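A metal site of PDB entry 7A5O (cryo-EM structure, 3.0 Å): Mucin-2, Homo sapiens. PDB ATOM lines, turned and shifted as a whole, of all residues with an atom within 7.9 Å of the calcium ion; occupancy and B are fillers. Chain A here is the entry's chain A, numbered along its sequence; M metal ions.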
ATOM      1  N   THR A  27      25.835   0.726   0.989  1.00  0.00           N
ATOM      2  CA  THR A  27      24.803   0.855  -0.024  1.00  0.00           C
ATOM      3  C   THR A  27      25.431   0.935  -1.410  1.00  0.00           C
ATOM      4  O   THR A  27      26.650   0.841  -1.586  1.00  0.00           O
ATOM      5  CB  THR A  27      23.949   2.094   0.230  1.00  0.00           C
ATOM      6  OG1 THR A  27      24.759   3.266   0.088  1.00  0.00           O
ATOM      7  CG2 THR A  27      23.395   2.070   1.639  1.00  0.00           C
ATOM      8  N   PHE A  28      24.589   1.132  -2.424  1.00  0.00           N
ATOM      9  CA  PHE A  28      25.090   1.362  -3.777  1.00  0.00           C
ATOM     10  C   PHE A  28      25.798   2.691  -3.947  1.00  0.00           C
ATOM     11  O   PHE A  28      26.467   2.892  -4.962  1.00  0.00           O
ATOM     12  CB  PHE A  28      23.949   1.310  -4.779  1.00  0.00           C
ATOM     13  CG  PHE A  28      23.356  -0.050  -4.999  1.00  0.00           C
ATOM     14  CD1 PHE A  28      24.023  -0.983  -5.762  1.00  0.00           C
ATOM     15  CD2 PHE A  28      22.113  -0.360  -4.496  1.00  0.00           C
ATOM     16  CE1 PHE A  28      23.481  -2.232  -5.992  1.00  0.00           C
ATOM     17  CE2 PHE A  28      21.558  -1.611  -4.727  1.00  0.00           C
ATOM     18  CZ  PHE A  28      22.250  -2.540  -5.463  1.00  0.00           C
ATOM     19  N   ASP A  29      25.671   3.601  -2.989  1.00  0.00           N
ATOM     20  CA  ASP A  29      26.231   4.940  -3.043  1.00  0.00           C
ATOM     21  C   ASP A  29      27.048   5.213  -1.796  1.00  0.00           C
ATOM     22  O   ASP A  29      26.873   6.217  -1.114  1.00  0.00           O
ATOM     23  CB  ASP A  29      25.129   5.980  -3.188  1.00  0.00           C
ATOM     24  CG  ASP A  29      24.383   5.847  -4.487  1.00  0.00           C
ATOM     25  OD1 ASP A  29      24.986   5.386  -5.471  1.00  0.00           O
ATOM     26  OD2 ASP A  29      23.187   6.195  -4.524  1.00  0.00           O
ATOM     27  N   ASP A  31      27.770   4.986   1.943  1.00  0.00           N
ATOM     28  CA  ASP A  31      26.912   4.904   3.132  1.00  0.00           C
ATOM     29  C   ASP A  31      27.176   3.633   3.935  1.00  0.00           C
ATOM     30  O   ASP A  31      26.337   2.732   4.029  1.00  0.00           O
ATOM     31  CB  ASP A  31      25.426   5.021   2.773  1.00  0.00           C
ATOM     32  CG  ASP A  31      25.056   6.384   2.255  1.00  0.00           C
ATOM     33  OD1 ASP A  31      25.718   7.361   2.662  1.00  0.00           O
ATOM     34  OD2 ASP A  31      24.101   6.479   1.460  1.00  0.00           O
ATOM     35  N   ASN A 143      17.138   4.804  -9.974  1.00  0.00           N
ATOM     36  CA  ASN A 143      15.950   5.405  -9.368  1.00  0.00           C
ATOM     37  C   ASN A 143      14.827   4.403  -9.092  1.00  0.00           C
ATOM     38  O   ASN A 143      13.687   4.813  -8.877  1.00  0.00           O
ATOM     39  CB  ASN A 143      15.358   6.557 -10.210  1.00  0.00           C
ATOM     40  CG  ASN A 143      16.235   7.806 -10.202  1.00  0.00           C
ATOM     41  OD1 ASN A 143      16.815   8.157  -9.180  1.00  0.00           O
ATOM     42  ND2 ASN A 143      16.276   8.489 -11.368  1.00  0.00           N
ATOM     43  N   CYS A 149      19.901  -1.586   0.759  1.00  0.00           N
ATOM     44  CA  CYS A 149      21.008  -1.070  -0.018  1.00  0.00           C
ATOM     45  C   CYS A 149      20.771   0.326  -0.570  1.00  0.00           C
ATOM     46  O   CYS A 149      21.494   0.749  -1.464  1.00  0.00           O
ATOM     47  CB  CYS A 149      21.318  -2.018  -1.176  1.00  0.00           C
ATOM     48  SG  CYS A 149      21.918  -3.640  -0.715  1.00  0.00           S
ATOM     49  N   GLY A 150      19.747   1.027  -0.089  1.00  0.00           N
ATOM     50  CA  GLY A 150      19.426   2.347  -0.579  1.00  0.00           C
ATOM     51  C   GLY A 150      18.833   2.316  -1.975  1.00  0.00           C
ATOM     52  O   GLY A 150      18.613   1.272  -2.585  1.00  0.00           O
ATOM     53  N   ASP A 151      18.553   3.514  -2.482  1.00  0.00           N
ATOM     54  CA  ASP A 151      18.222   3.654  -3.882  1.00  0.00           C
ATOM     55  C   ASP A 151      19.496   3.828  -4.710  1.00  0.00           C
ATOM     56  O   ASP A 151      20.602   3.949  -4.176  1.00  0.00           O
ATOM     57  CB  ASP A 151      17.222   4.792  -4.100  1.00  0.00           C
ATOM     58  CG  ASP A 151      17.712   6.133  -3.540  1.00  0.00           C
ATOM     59  OD1 ASP A 151      18.781   6.181  -2.896  1.00  0.00           O
ATOM     60  OD2 ASP A 151      16.999   7.134  -3.740  1.00  0.00           O
ATOM     61  N   TYR A 152      19.333   3.823  -6.028  1.00  0.00           N
ATOM     62  CA  TYR A 152      20.472   3.688  -6.924  1.00  0.00           C
ATOM     63  C   TYR A 152      20.488   4.875  -7.869  1.00  0.00           C
ATOM     64  O   TYR A 152      20.567   4.742  -9.087  1.00  0.00           O
ATOM     65  CB  TYR A 152      20.389   2.313  -7.611  1.00  0.00           C
ATOM     66  CG  TYR A 152      21.512   1.904  -8.531  1.00  0.00           C
ATOM     67  CD1 TYR A 152      22.797   1.732  -8.049  1.00  0.00           C
ATOM     68  CD2 TYR A 152      21.264   1.529  -9.841  1.00  0.00           C
ATOM     69  CE1 TYR A 152      23.830   1.333  -8.857  1.00  0.00           C
ATOM     70  CE2 TYR A 152      22.289   1.104 -10.667  1.00  0.00           C
ATOM     71  CZ  TYR A 152      23.562   1.013 -10.163  1.00  0.00           C
ATOM     72  OH  TYR A 152      24.599   0.590 -10.963  1.00  0.00           O
ATOM     73  N   ASN A 153      20.391   6.067  -7.278  1.00  0.00           N
ATOM     74  CA  ASN A 153      20.422   7.337  -7.977  1.00  0.00           C
ATOM     75  C   ASN A 153      21.821   7.904  -8.167  1.00  0.00           C
ATOM     76  O   ASN A 153      22.025   8.746  -9.054  1.00  0.00           O
ATOM     77  CB  ASN A 153      19.538   8.357  -7.236  1.00  0.00           C
ATOM     78  CG  ASN A 153      19.952   8.569  -5.771  1.00  0.00           C
ATOM     79  OD1 ASN A 153      20.955   8.034  -5.299  1.00  0.00           O
ATOM     80  ND2 ASN A 153      19.158   9.359  -5.053  1.00  0.00           N
ATOM     81  N   GLY A 154      22.795   7.460  -7.367  1.00  0.00           N
ATOM     82  CA  GLY A 154      24.136   7.979  -7.440  1.00  0.00           C
ATOM     83  C   GLY A 154      24.463   9.051  -6.420  1.00  0.00           C
ATOM     84  O   GLY A 154      25.626   9.455  -6.328  1.00  0.00           O
ATOM     85  N   LEU A 155      23.488   9.498  -5.643  1.00  0.00           N
ATOM     86  CA  LEU A 155      23.685  10.604  -4.714  1.00  0.00           C
ATOM     87  C   LEU A 155      24.047  10.058  -3.327  1.00  0.00           C
ATOM     88  O   LEU A 155      23.307   9.242  -2.768  1.00  0.00           O
ATOM     89  CB  LEU A 155      22.435  11.470  -4.642  1.00  0.00           C
ATOM     90  N   GLN A 156      25.179  10.521  -2.793  1.00  0.00           N
ATOM     91  CA  GLN A 156      25.665  10.142  -1.479  1.00  0.00           C
ATOM     92  C   GLN A 156      24.725  10.610  -0.367  1.00  0.00           C
ATOM     93  O   GLN A 156      24.602  11.807  -0.118  1.00  0.00           O
ATOM     94  CB  GLN A 156      27.043  10.753  -1.239  1.00  0.00           C
ATOM     95  CG  GLN A 156      27.687  10.412   0.093  1.00  0.00           C
ATOM     96  CD  GLN A 156      28.128   8.975   0.167  1.00  0.00           C
ATOM     97  OE1 GLN A 156      28.695   8.435  -0.785  1.00  0.00           O
ATOM     98  NE2 GLN A 156      27.898   8.342   1.308  1.00  0.00           N
ATOM     99  N   SER A 157      24.055   9.653   0.295  1.00  0.00           N
ATOM    100  CA  SER A 157      23.254   9.853   1.511  1.00  0.00           C
ATOM    101  C   SER A 157      22.119  10.852   1.338  1.00  0.00           C
ATOM    102  O   SER A 157      21.669  11.455   2.317  1.00  0.00           O
ATOM    103  CB  SER A 157      24.140  10.276   2.689  1.00  0.00           C
ATOM    104  OG  SER A 157      23.353  10.503   3.850  1.00  0.00           O
ATOM    105  N   TYR A 158      21.613  11.042   0.110  1.00  0.00           N
ATOM    106  CA  TYR A 158      20.638  12.098  -0.120  1.00  0.00           C
ATOM    107  C   TYR A 158      19.239  11.663   0.303  1.00  0.00           C
ATOM    108  O   TYR A 158      18.663  12.218   1.242  1.00  0.00           O
ATOM    109  CB  TYR A 158      20.650  12.508  -1.594  1.00  0.00           C
ATOM    110  N   SER A 159      18.689  10.659  -0.367  1.00  0.00           N
ATOM    111  CA  SER A 159      17.307  10.242  -0.119  1.00  0.00           C
ATOM    112  C   SER A 159      17.201   9.019   0.769  1.00  0.00           C
ATOM    113  O   SER A 159      16.085   8.613   1.095  1.00  0.00           O
ATOM    114  CB  SER A 159      16.597   9.975  -1.455  1.00  0.00           C
ATOM    115  OG  SER A 159      17.188   8.877  -2.122  1.00  0.00           O
ATOM    116  N   GLU A 160      18.318   8.415   1.170  1.00  0.00           N
ATOM    117  CA  GLU A 160      18.256   7.283   2.084  1.00  0.00           C
ATOM    118  C   GLU A 160      17.995   7.742   3.503  1.00  0.00           C
ATOM    119  O   GLU A 160      17.115   7.209   4.190  1.00  0.00           O
ATOM    120  CB  GLU A 160      19.552   6.467   2.033  1.00  0.00           C
ATOM    121  CG  GLU A 160      19.846   5.772   0.713  1.00  0.00           C
ATOM    122  CD  GLU A 160      20.620   6.653  -0.259  1.00  0.00           C
ATOM    123  OE1 GLU A 160      20.955   7.794   0.116  1.00  0.00           O
ATOM    124  OE2 GLU A 160      20.910   6.190  -1.385  1.00  0.00           O
ATOM    125  N   PHE A 161      18.750   8.737   3.966  1.00  0.00           N
ATOM    126  CA  PHE A 161      18.701   9.162   5.358  1.00  0.00           C
ATOM    127  C   PHE A 161      17.978  10.480   5.575  1.00  0.00           C
ATOM    128  O   PHE A 161      17.482  10.714   6.684  1.00  0.00           O
ATOM    129  CB  PHE A 161      20.122   9.282   5.932  1.00  0.00           C
ATOM    130  CG  PHE A 161      20.835   7.963   6.111  1.00  0.00           C
ATOM    131  CD1 PHE A 161      20.137   6.762   6.101  1.00  0.00           C
ATOM    132  CD2 PHE A 161      22.208   7.925   6.312  1.00  0.00           C
ATOM    133  CE1 PHE A 161      20.790   5.566   6.275  1.00  0.00           C
ATOM    134  CE2 PHE A 161      22.861   6.730   6.487  1.00  0.00           C
ATOM    135  CZ  PHE A 161      22.153   5.544   6.464  1.00  0.00           C
HETATM  136 CA    CA M   1      21.019   8.056  -2.759  1.00  0.00          CA
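Asp 29 touches the calcium ion. Ser 159 touches the calcium ion. Within 4 Å of the calcium ion: Asp 29, Asp 151, Asn 153, Leu 155, Ser 159 and Glu 160.
OE2 of Glu 160 binds the calcium ion (2.3 Å). OD1 of Asn 153 is bound to the calcium ion, 2.5 Å away. O of Leu 155 binds the calcium ion (2.6 Å). The calcium ion is bound by OE1 of Glu 160 (2.9 Å). Slightly farther from the calcium ion lies the side-chain carboxylate (OD1) of Asp 151 (2.9 Å).
OD1 of Asp 151 lies close to OE2 of Glu 160 (2.6 Å). N of Tyr 158 lies close to OE1 of Glu 160 (3.3 Å). ND2 of Asn 153 lies within hydrogen-bond range of OD2 of Asp 151 (3.4 Å). The side-chain amide oxygen (OD1) of Asn 153 sits close to the side-chain carboxylate (OD2) of Asp 29, at 3.0 Å. OG of Ser 159 lies close to OD1 of Asp 151 (3.2 Å). The side-chain amide oxygen (OE1) of Gln 156 sits close to the backbone carbonyl oxygen (O) of Asp 29. The side-chain carboxylate of Asp 29 lies within hydrogen-bond range of the backbone NH of Gly 154 (3.1 Å). OG1 of Thr 27 lies close to N of Asp 29.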
